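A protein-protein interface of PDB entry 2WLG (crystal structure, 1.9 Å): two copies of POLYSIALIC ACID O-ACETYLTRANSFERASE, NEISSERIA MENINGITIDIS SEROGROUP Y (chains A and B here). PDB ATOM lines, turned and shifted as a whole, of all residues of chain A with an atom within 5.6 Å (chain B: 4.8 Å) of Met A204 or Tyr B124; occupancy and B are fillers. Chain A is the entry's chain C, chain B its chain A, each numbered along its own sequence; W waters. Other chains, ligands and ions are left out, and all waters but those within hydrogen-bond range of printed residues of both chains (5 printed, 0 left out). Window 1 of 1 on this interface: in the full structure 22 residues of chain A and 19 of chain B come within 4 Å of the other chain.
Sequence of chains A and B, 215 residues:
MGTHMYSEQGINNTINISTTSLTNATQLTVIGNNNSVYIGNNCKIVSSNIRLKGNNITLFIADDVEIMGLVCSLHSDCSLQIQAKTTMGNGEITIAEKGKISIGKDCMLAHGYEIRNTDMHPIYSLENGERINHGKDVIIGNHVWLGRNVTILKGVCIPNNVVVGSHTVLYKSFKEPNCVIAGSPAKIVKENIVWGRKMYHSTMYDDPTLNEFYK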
ATOM      1  N   ASN A 192      17.504  -0.706 -17.673  1.00  0.00           N
ATOM      2  CA  ASN A 192      18.839  -0.346 -17.200  1.00  0.00           C
ATOM      3  C   ASN A 192      18.788   0.646 -16.054  1.00  0.00           C
ATOM      4  O   ASN A 192      19.510   1.647 -16.058  1.00  0.00           O
ATOM      5  CB  ASN A 192      19.636   0.274 -18.333  1.00  0.00           C
ATOM      6  CG  ASN A 192      19.802  -0.647 -19.490  1.00  0.00           C
ATOM      7  OD1 ASN A 192      20.002  -1.860 -19.317  1.00  0.00           O
ATOM      8  ND2 ASN A 192      19.757  -0.093 -20.698  1.00  0.00           N
ATOM      9  N   ILE A 193      17.958   0.356 -15.062  1.00  0.00           N
ATOM     10  CA  ILE A 193      17.865   1.204 -13.890  1.00  0.00           C
ATOM     11  C   ILE A 193      18.072   0.435 -12.604  1.00  0.00           C
ATOM     12  O   ILE A 193      18.154  -0.796 -12.595  1.00  0.00           O
ATOM     13  CB  ILE A 193      16.515   1.972 -13.839  1.00  0.00           C
ATOM     14  CG1 ILE A 193      15.329   1.012 -13.893  1.00  0.00           C
ATOM     15  CG2 ILE A 193      16.403   2.916 -14.998  1.00  0.00           C
ATOM     16  CD1 ILE A 193      14.970   0.409 -12.586  1.00  0.00           C
ATOM     17  N   VAL A 194      18.208   1.171 -11.512  1.00  0.00           N
ATOM     18  CA  VAL A 194      18.162   0.570 -10.176  1.00  0.00           C
ATOM     19  C   VAL A 194      17.464   1.577  -9.275  1.00  0.00           C
ATOM     20  O   VAL A 194      17.739   2.784  -9.375  1.00  0.00           O
ATOM     21  CB  VAL A 194      19.583   0.211  -9.608  1.00  0.00           C
ATOM     22  CG1 VAL A 194      20.459   1.438  -9.495  1.00  0.00           C
ATOM     23  CG2 VAL A 194      19.457  -0.463  -8.254  1.00  0.00           C
ATOM     24  N   TRP A 195      16.570   1.108  -8.408  1.00  0.00           N
ATOM     25  CA  TRP A 195      15.870   2.018  -7.497  1.00  0.00           C
ATOM     26  C   TRP A 195      16.481   1.898  -6.107  1.00  0.00           C
ATOM     27  O   TRP A 195      17.164   0.913  -5.794  1.00  0.00           O
ATOM     28  CB  TRP A 195      14.366   1.728  -7.449  1.00  0.00           C
ATOM     29  CG  TRP A 195      14.022   0.349  -6.892  1.00  0.00           C
ATOM     30  CD1 TRP A 195      13.854  -0.798  -7.612  1.00  0.00           C
ATOM     31  CD2 TRP A 195      13.824  -0.013  -5.511  1.00  0.00           C
ATOM     32  NE1 TRP A 195      13.559  -1.843  -6.779  1.00  0.00           N
ATOM     33  CE2 TRP A 195      13.525  -1.393  -5.483  1.00  0.00           C
ATOM     34  CE3 TRP A 195      13.830   0.699  -4.310  1.00  0.00           C
ATOM     35  CZ2 TRP A 195      13.278  -2.080  -4.300  1.00  0.00           C
ATOM     36  CZ3 TRP A 195      13.594   0.011  -3.127  1.00  0.00           C
ATOM     37  CH2 TRP A 195      13.321  -1.365  -3.133  1.00  0.00           C
ATOM     38  N   GLY A 196      16.269   2.916  -5.282  1.00  0.00           N
ATOM     39  CA  GLY A 196      16.686   2.869  -3.874  1.00  0.00           C
ATOM     40  C   GLY A 196      15.633   3.507  -2.993  1.00  0.00           C
ATOM     41  O   GLY A 196      14.631   4.019  -3.483  1.00  0.00           O
ATOM     42  N   LYS A 198      16.175   6.082  -0.576  1.00  0.00           N
ATOM     43  CA  LYS A 198      16.493   7.390   0.026  1.00  0.00           C
ATOM     44  C   LYS A 198      16.674   8.486  -0.997  1.00  0.00           C
ATOM     45  O   LYS A 198      17.694   8.527  -1.693  1.00  0.00           O
ATOM     46  CB  LYS A 198      17.800   7.298   0.828  1.00  0.00           C
ATOM     47  CG  LYS A 198      17.819   6.248   1.885  1.00  0.00           C
ATOM     48  CD  LYS A 198      16.832   6.562   2.982  1.00  0.00           C
ATOM     49  CE  LYS A 198      17.131   5.781   4.252  1.00  0.00           C
ATOM     50  NZ  LYS A 198      16.217   4.602   4.436  1.00  0.00           N
ATOM     51  N   HIS A 201      20.066  10.824  -1.231  1.00  0.00           N
ATOM     52  CA  HIS A 201      21.331  10.449  -1.877  1.00  0.00           C
ATOM     53  C   HIS A 201      21.548  11.053  -3.268  1.00  0.00           C
ATOM     54  O   HIS A 201      20.606  11.259  -4.060  1.00  0.00           O
ATOM     55  CB  HIS A 201      21.501   8.936  -1.966  1.00  0.00           C
ATOM     56  CG  HIS A 201      21.992   8.296  -0.710  1.00  0.00           C
ATOM     57  ND1 HIS A 201      23.074   8.785   0.003  1.00  0.00           N
ATOM     58  CD2 HIS A 201      21.529   7.223  -0.017  1.00  0.00           C
ATOM     59  CE1 HIS A 201      23.277   8.011   1.060  1.00  0.00           C
ATOM     60  NE2 HIS A 201      22.351   7.059   1.074  1.00  0.00           N
ATOM     61  N   SER A 202      22.803  11.393  -3.543  1.00  0.00           N
ATOM     62  CA  SER A 202      23.155  11.992  -4.808  1.00  0.00           C
ATOM     63  C   SER A 202      23.036  10.976  -5.938  1.00  0.00           C
ATOM     64  O   SER A 202      22.435  11.263  -6.991  1.00  0.00           O
ATOM     65  CB  SER A 202      24.578  12.554  -4.775  1.00  0.00           C
ATOM     66  OG  SER A 202      24.730  13.479  -3.723  1.00  0.00           O
ATOM     67  N   THR A 203      23.636   9.807  -5.735  1.00  0.00           N
ATOM     68  CA  THR A 203      23.792   8.838  -6.812  1.00  0.00           C
ATOM     69  C   THR A 203      23.652   7.425  -6.263  1.00  0.00           C
ATOM     70  O   THR A 203      23.671   7.197  -5.042  1.00  0.00           O
ATOM     71  CB  THR A 203      25.182   8.947  -7.493  1.00  0.00           C
ATOM     72  OG1 THR A 203      26.149   8.394  -6.607  1.00  0.00           O
ATOM     73  CG2 THR A 203      25.578  10.406  -7.859  1.00  0.00           C
ATOM     74  N   MET A 204      23.558   6.442  -7.150  1.00  0.00           N
ATOM     75  CA  MET A 204      23.410   5.071  -6.700  1.00  0.00           C
ATOM     76  C   MET A 204      24.615   4.625  -5.890  1.00  0.00           C
ATOM     77  O   MET A 204      24.499   3.793  -4.973  1.00  0.00           O
ATOM     78  CB  MET A 204      23.170   4.122  -7.881  1.00  0.00           C
ATOM     79  CG  MET A 204      24.383   3.712  -8.659  1.00  0.00           C
ATOM     80  SD  MET A 204      23.833   2.852 -10.161  1.00  0.00           S
ATOM     81  CE  MET A 204      25.367   2.714 -11.053  1.00  0.00           C
ATOM     82  N   TYR A 205      25.773   5.204  -6.204  1.00  0.00           N
ATOM     83  CA  TYR A 205      27.013   4.848  -5.526  1.00  0.00           C
ATOM     84  C   TYR A 205      27.021   5.229  -4.068  1.00  0.00           C
ATOM     85  O   TYR A 205      27.825   4.699  -3.288  1.00  0.00           O
ATOM     86  CB  TYR A 205      28.191   5.536  -6.205  1.00  0.00           C
ATOM     87  CG  TYR A 205      28.291   5.166  -7.657  1.00  0.00           C
ATOM     88  CD1 TYR A 205      28.017   6.090  -8.646  1.00  0.00           C
ATOM     89  CD2 TYR A 205      28.647   3.878  -8.037  1.00  0.00           C
ATOM     90  CE1 TYR A 205      28.105   5.751  -9.987  1.00  0.00           C
ATOM     91  CE2 TYR A 205      28.745   3.536  -9.391  1.00  0.00           C
ATOM     92  CZ  TYR A 205      28.455   4.479 -10.348  1.00  0.00           C
ATOM     93  OH  TYR A 205      28.544   4.152 -11.682  1.00  0.00           O
ATOM     94  N   ASP A 206      26.128   6.134  -3.692  1.00  0.00           N
ATOM     95  CA  ASP A 206      26.061   6.642  -2.331  1.00  0.00           C
ATOM     96  C   ASP A 206      25.273   5.734  -1.416  1.00  0.00           C
ATOM     97  O   ASP A 206      25.298   5.888  -0.186  1.00  0.00           O
ATOM     98  CB  ASP A 206      25.467   8.070  -2.318  1.00  0.00           C
ATOM     99  CG  ASP A 206      26.449   9.081  -2.831  1.00  0.00           C
ATOM    100  OD1 ASP A 206      27.435   9.295  -2.111  1.00  0.00           O
ATOM    101  OD2 ASP A 206      26.266   9.605  -3.981  1.00  0.00           O
ATOM    102  N   ASP A 207      24.615   4.749  -2.021  1.00  0.00           N
ATOM    103  CA  ASP A 207      23.735   3.863  -1.290  1.00  0.00           C
ATOM    104  C   ASP A 207      24.324   2.456  -1.289  1.00  0.00           C
ATOM    105  O   ASP A 207      24.281   1.776  -2.297  1.00  0.00           O
ATOM    106  CB  ASP A 207      22.346   3.867  -1.928  1.00  0.00           C
ATOM    107  CG  ASP A 207      21.349   3.007  -1.148  1.00  0.00           C
ATOM    108  OD1 ASP A 207      21.798   2.211  -0.302  1.00  0.00           O
ATOM    109  OD2 ASP A 207      20.139   3.107  -1.428  1.00  0.00           O
ATOM    110  N   PRO A 208      24.907   2.045  -0.165  1.00  0.00           N
ATOM    111  CA  PRO A 208      25.708   0.825  -0.131  1.00  0.00           C
ATOM    112  C   PRO A 208      24.865  -0.408  -0.366  1.00  0.00           C
ATOM    113  O   PRO A 208      25.406  -1.450  -0.706  1.00  0.00           O
ATOM    114  CB  PRO A 208      26.294   0.810   1.295  1.00  0.00           C
ATOM    115  CG  PRO A 208      26.068   2.176   1.837  1.00  0.00           C
ATOM    116  CD  PRO A 208      24.971   2.810   1.090  1.00  0.00           C
ATOM    117  N   LEU A 210      22.953  -0.839  -2.737  1.00  0.00           N
ATOM    118  CA  LEU A 210      22.717  -1.022  -4.176  1.00  0.00           C
ATOM    119  C   LEU A 210      23.923  -1.591  -4.945  1.00  0.00           C
ATOM    120  O   LEU A 210      23.827  -1.826  -6.174  1.00  0.00           O
ATOM    121  CB  LEU A 210      22.252   0.252  -4.835  1.00  0.00           C
ATOM    122  CG  LEU A 210      21.035   0.913  -4.201  1.00  0.00           C
ATOM    123  CD1 LEU A 210      20.662   2.177  -4.970  1.00  0.00           C
ATOM    124  CD2 LEU A 210      19.888  -0.075  -4.163  1.00  0.00           C
ATOM    125  N   ASN A 211      25.009  -1.824  -4.206  1.00  0.00           N
ATOM    126  CA  ASN A 211      26.294  -2.276  -4.774  1.00  0.00           C
ATOM    127  C   ASN A 211      26.089  -3.584  -5.563  1.00  0.00           C
ATOM    128  O   ASN A 211      26.691  -3.792  -6.619  1.00  0.00           O
ATOM    129  CB  ASN A 211      27.336  -2.506  -3.666  1.00  0.00           C
ATOM    130  CG  ASN A 211      27.927  -1.198  -3.080  1.00  0.00           C
ATOM    131  OD1 ASN A 211      29.034  -1.219  -2.506  1.00  0.00           O
ATOM    132  ND2 ASN A 211      27.205  -0.083  -3.192  1.00  0.00           N
ATOM    133  N   TYR A 214      24.799  -3.302  -9.548  1.00  0.00           N
ATOM    134  CA  TYR A 214      25.568  -2.763 -10.669  1.00  0.00           C
ATOM    135  C   TYR A 214      27.004  -3.235 -10.570  1.00  0.00           C
ATOM    136  O   TYR A 214      27.393  -3.896  -9.608  1.00  0.00           O
ATOM    137  CB  TYR A 214      25.510  -1.217 -10.697  1.00  0.00           C
ATOM    138  CG  TYR A 214      26.124  -0.567  -9.487  1.00  0.00           C
ATOM    139  CD1 TYR A 214      25.332  -0.121  -8.437  1.00  0.00           C
ATOM    140  CD2 TYR A 214      27.501  -0.429  -9.379  1.00  0.00           C
ATOM    141  CE1 TYR A 214      25.885   0.450  -7.316  1.00  0.00           C
ATOM    142  CE2 TYR A 214      28.068   0.152  -8.263  1.00  0.00           C
ATOM    143  CZ  TYR A 214      27.250   0.590  -7.228  1.00  0.00           C
ATOM    144  OH  TYR A 214      27.813   1.154  -6.120  1.00  0.00           O
ATOM    145  N   PRO B 122      14.065   7.215  -5.012  1.00  0.00           N
ATOM    146  CA  PRO B 122      14.853   7.432  -6.205  1.00  0.00           C
ATOM    147  C   PRO B 122      14.966   6.278  -7.190  1.00  0.00           C
ATOM    148  O   PRO B 122      15.005   5.122  -6.806  1.00  0.00           O
ATOM    149  CB  PRO B 122      16.240   7.750  -5.649  1.00  0.00           C
ATOM    150  CG  PRO B 122      16.313   6.935  -4.406  1.00  0.00           C
ATOM    151  CD  PRO B 122      14.911   6.953  -3.828  1.00  0.00           C
ATOM    152  N   ILE B 123      15.031   6.627  -8.470  1.00  0.00           N
ATOM    153  CA  ILE B 123      15.442   5.687  -9.497  1.00  0.00           C
ATOM    154  C   ILE B 123      16.707   6.252 -10.166  1.00  0.00           C
ATOM    155  O   ILE B 123      16.773   7.445 -10.507  1.00  0.00           O
ATOM    156  CB  ILE B 123      14.355   5.439 -10.516  1.00  0.00           C
ATOM    157  CG1 ILE B 123      13.102   4.869  -9.840  1.00  0.00           C
ATOM    158  CG2 ILE B 123      14.840   4.484 -11.578  1.00  0.00           C
ATOM    159  CD1 ILE B 123      11.932   4.766 -10.822  1.00  0.00           C
ATOM    160  N   TYR B 124      17.710   5.394 -10.306  1.00  0.00           N
ATOM    161  CA  TYR B 124      18.988   5.776 -10.916  1.00  0.00           C
ATOM    162  C   TYR B 124      19.247   5.034 -12.194  1.00  0.00           C
ATOM    163  O   TYR B 124      18.896   3.861 -12.352  1.00  0.00           O
ATOM    164  CB  TYR B 124      20.156   5.472  -9.987  1.00  0.00           C
ATOM    165  CG  TYR B 124      20.007   5.949  -8.572  1.00  0.00           C
ATOM    166  CD1 TYR B 124      20.321   7.248  -8.201  1.00  0.00           C
ATOM    167  CD2 TYR B 124      19.617   5.072  -7.575  1.00  0.00           C
ATOM    168  CE1 TYR B 124      20.193   7.664  -6.871  1.00  0.00           C
ATOM    169  CE2 TYR B 124      19.487   5.481  -6.275  1.00  0.00           C
ATOM    170  CZ  TYR B 124      19.765   6.770  -5.922  1.00  0.00           C
ATOM    171  OH  TYR B 124      19.613   7.100  -4.571  1.00  0.00           O
ATOM    172  N   SER B 125      19.907   5.709 -13.118  1.00  0.00           N
ATOM    173  CA  SER B 125      20.336   5.056 -14.346  1.00  0.00           C
ATOM    174  C   SER B 125      21.651   4.305 -14.132  1.00  0.00           C
ATOM    175  O   SER B 125      22.591   4.853 -13.561  1.00  0.00           O
ATOM    176  CB  SER B 125      20.512   6.079 -15.450  1.00  0.00           C
ATOM    177  OG  SER B 125      21.140   5.437 -16.539  1.00  0.00           O
ATOM    178  N   LEU B 126      21.689   3.050 -14.561  1.00  0.00           N
ATOM    179  CA  LEU B 126      22.904   2.251 -14.510  1.00  0.00           C
ATOM    180  C   LEU B 126      24.002   2.759 -15.462  1.00  0.00           C
ATOM    181  O   LEU B 126      25.151   2.358 -15.332  1.00  0.00           O
ATOM    182  CB  LEU B 126      22.604   0.768 -14.824  1.00  0.00           C
ATOM    183  CG  LEU B 126      21.718   0.041 -13.803  1.00  0.00           C
ATOM    184  CD1 LEU B 126      21.446  -1.396 -14.248  1.00  0.00           C
ATOM    185  CD2 LEU B 126      22.362   0.055 -12.421  1.00  0.00           C
ATOM    186  N   GLY B 129      24.858   6.123 -12.916  1.00  0.00           N
ATOM    187  CA  GLY B 129      24.517   6.239 -11.517  1.00  0.00           C
ATOM    188  C   GLY B 129      23.612   7.378 -11.070  1.00  0.00           C
ATOM    189  O   GLY B 129      23.294   7.488  -9.865  1.00  0.00           O
ATOM    190  N   GLU B 130      23.221   8.228 -12.003  1.00  0.00           N
ATOM    191  CA  GLU B 130      22.530   9.447 -11.663  1.00  0.00           C
ATOM    192  C   GLU B 130      21.039   9.205 -11.523  1.00  0.00           C
ATOM    193  O   GLU B 130      20.451   8.346 -12.210  1.00  0.00           O
ATOM    194  CB  GLU B 130      22.804  10.532 -12.689  1.00  0.00           C
ATOM    195  CG  GLU B 130      24.283  10.862 -12.861  1.00  0.00           C
ATOM    196  CD  GLU B 130      24.892  11.694 -11.741  1.00  0.00           C
ATOM    197  OE1 GLU B 130      24.162  12.412 -11.051  1.00  0.00           O
ATOM    198  OE2 GLU B 130      26.138  11.695 -11.612  1.00  0.00           O
ATOM    199  N   ARG B 131      20.443   9.975 -10.623  1.00  0.00           N
ATOM    200  CA  ARG B 131      19.005   9.885 -10.372  1.00  0.00           C
ATOM    201  C   ARG B 131      18.252  10.442 -11.570  1.00  0.00           C
ATOM    202  O   ARG B 131      18.543  11.534 -12.003  1.00  0.00           O
ATOM    203  CB  ARG B 131      18.636  10.652  -9.104  1.00  0.00           C
ATOM    204  CG  ARG B 131      17.164  10.532  -8.791  1.00  0.00           C
ATOM    205  CD  ARG B 131      16.741  11.219  -7.525  1.00  0.00           C
ATOM    206  NE  ARG B 131      15.287  11.097  -7.420  1.00  0.00           N
ATOM    207  CZ  ARG B 131      14.537  11.742  -6.532  1.00  0.00           C
ATOM    208  NH1 ARG B 131      15.091  12.568  -5.683  1.00  0.00           N
ATOM    209  NH2 ARG B 131      13.215  11.552  -6.513  1.00  0.00           N
ATOM    210  N   ILE B 132      17.285   9.685 -12.081  1.00  0.00           N
ATOM    211  CA  ILE B 132      16.487  10.091 -13.237  1.00  0.00           C
ATOM    212  C   ILE B 132      15.041  10.486 -12.972  1.00  0.00           C
ATOM    213  O   ILE B 132      14.340  10.896 -13.915  1.00  0.00           O
ATOM    214  CB  ILE B 132      16.443   9.009 -14.308  1.00  0.00           C
ATOM    215  CG1 ILE B 132      15.797   7.722 -13.758  1.00  0.00           C
ATOM    216  CG2 ILE B 132      17.867   8.787 -14.892  1.00  0.00           C
ATOM    217  CD1 ILE B 132      15.563   6.688 -14.808  1.00  0.00           C
HETATM  218  O   HOH W   1      18.722   5.355  -2.243  1.00  0.00           O
HETATM  219  O   HOH W   2      19.035   3.980 -17.799  1.00  0.00           O
HETATM  220  O   HOH W   3      17.841  13.127  -5.044  1.00  0.00           O
HETATM  221  O   HOH W   4      18.564   9.606  -4.316  1.00  0.00           O
HETATM  222  O   HOH W   5      22.084  12.112  -9.447  1.00  0.00           O
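The backbone carbonyl oxygen of Val A194 sits at hydrogen-bond distance from the backbone NH of Tyr B124, at 2.8 Å.
The backbone NH (N) of Leu B126 sits at hydrogen-bond distance from the backbone carbonyl oxygen (O) of Asn A192 (3.0 Å).
The backbone NH of Gly A196 sits at hydrogen-bond distance from the backbone carbonyl oxygen of Pro B122, at 3.0 Å.
N of Met A204 lies within hydrogen-bond range of O of Gly B129.
The side-chain amide nitrogen of Asn A211 lies within hydrogen-bond range of the side-chain hydroxyl of Tyr A214 (3.2 Å).
N of Ser B125 is in hydrogen-bond range of O of Glu B130 (2.8 Å).
OG1 of Thr A203 lies within hydrogen-bond range of OD2 of Asp A206.
The backbone NH of Ile B132 is in hydrogen-bond range of the backbone carbonyl oxygen of Ile B123, at 2.8 Å.
O of Asp A206 sits close to NE2 of His A201.
OG1 of Thr A203 sits close to N of Tyr A205, at 3.2 Å.
Among the printed residues, pairs that only touch across the chains: Asn A192 with Ser B125 (3.9 Å), Ile A193 with Ile B123 (3.8 Å), Ile A193 with Tyr B124 (3.2 Å), Ile A193 with Leu B126 (3.7 Å), Ile A193 with Ile B132 (3.9 Å), Val A194 with Ile B123 (3.7 Å), Val A194 with Leu B126 (3.8 Å), Trp A195 with Pro B122 (3.3 Å), Lys A198 with Pro B122 (3.4 Å), Lys A198 with Tyr B124 (3.7 Å), His A201 with Tyr B124 (3.7 Å), Thr A203 with Tyr B124 (3.5 Å), Thr A203 with Gly B129 (3.4 Å), Met A204 with Tyr B124 (3.5 Å), Met A204 with Leu B126 (3.9 Å), Tyr A205 with Gly B129 (3.9 Å), Leu A210 with Tyr B124 (3.7 Å) and Tyr A214 with Leu B126 (3.8 Å).
Of the printed residues of chain B, Ile A193 touches Ile B123 (3.8 Å), Tyr B124 (3.2 Å), Leu B126 (3.7 Å) and Ile B132 (3.9 Å).
Of the printed residues of chain B, Trp A195 touches Pro B122 (3.3 Å).
Ser A202 touches none of the printed residues of chain B.
Met A204 touches just these residues of chain B: Tyr B124, Leu B126 and Gly B129.
Printed residues of chain A within 4 Å of Ile B123: Ile A193 and Val A194.
Tyr B124 touches just these residues of chain A: Ile A193 (3.2 Å), Val A194 (2.8 Å), Lys A198 (3.7 Å), His A201 (3.7 Å), Thr A203 (3.5 Å), Met A204 (3.5 Å) and Leu A210 (3.7 Å).
Printed residues of chain A within 4 Å of Ile B132: Ile A193.
The nearest residue of chain B that does not touch Met A204 is Ser B125 (4.1 Å).
Of the 17 printed residues of chain A, 12 touch a printed residue of chain B.
Printed residues of chain A that touch a printed residue of chain B: Asn A192, Ile A193, Val A194, Trp A195, Gly A196, Lys A198, His A201, Thr A203, Met A204, Tyr A205, Leu A210 and Tyr A214.
Hydrophobic or aromatic side chains of chain A that line the printed part of chain B: Ile A193, Val A194, Trp A195, His A201, Met A204, Tyr A205, Leu A210 and Tyr A214.
Of the 9 printed residues of chain B, 7 touch a printed residue of chain A.
Printed residues of chain B that touch a printed residue of chain A: Pro B122, Ile B123, Tyr B124, Ser B125, Leu B126, Gly B129 and Ile B132.
Hydrophobic or aromatic side chains of chain B that line the printed part of chain A: Pro B122, Ile B123, Tyr B124, Leu B126 and Ile B132.
Among the printed residues, 22 pairs touch across the chains.
No position is printed for both chains.
Water W5 lies within hydrogen-bond range of the backbone carbonyl oxygen of Ser A202 (2.6 Å), the side-chain carboxylate of Glu B130 (2.6 Å) and the backbone NH of Arg B131 (2.9 Å).
Water W4 lies within hydrogen-bond range of the backbone carbonyl oxygen (O) of His A201 (2.6 Å), the side-chain hydroxyl (OH) of Tyr B124 (2.7 Å) and the backbone carbonyl oxygen (O) of Lys A198 (3.0 Å).
Water W1 lies within hydrogen-bond range of OD2 of Asp A207 (2.8 Å), OH of Tyr B124 (3.0 Å) and N of Lys A198 (3.1 Å).
Water W2 lies within hydrogen-bond range of OG of Ser B125 (2.9 Å) and O of Asn A192 (2.9 Å).
Water W3 lies within hydrogen-bond range of the guanidinium group of Arg B131 (2.9 Å) and the backbone carbonyl oxygen of His A201 (3.5 Å).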
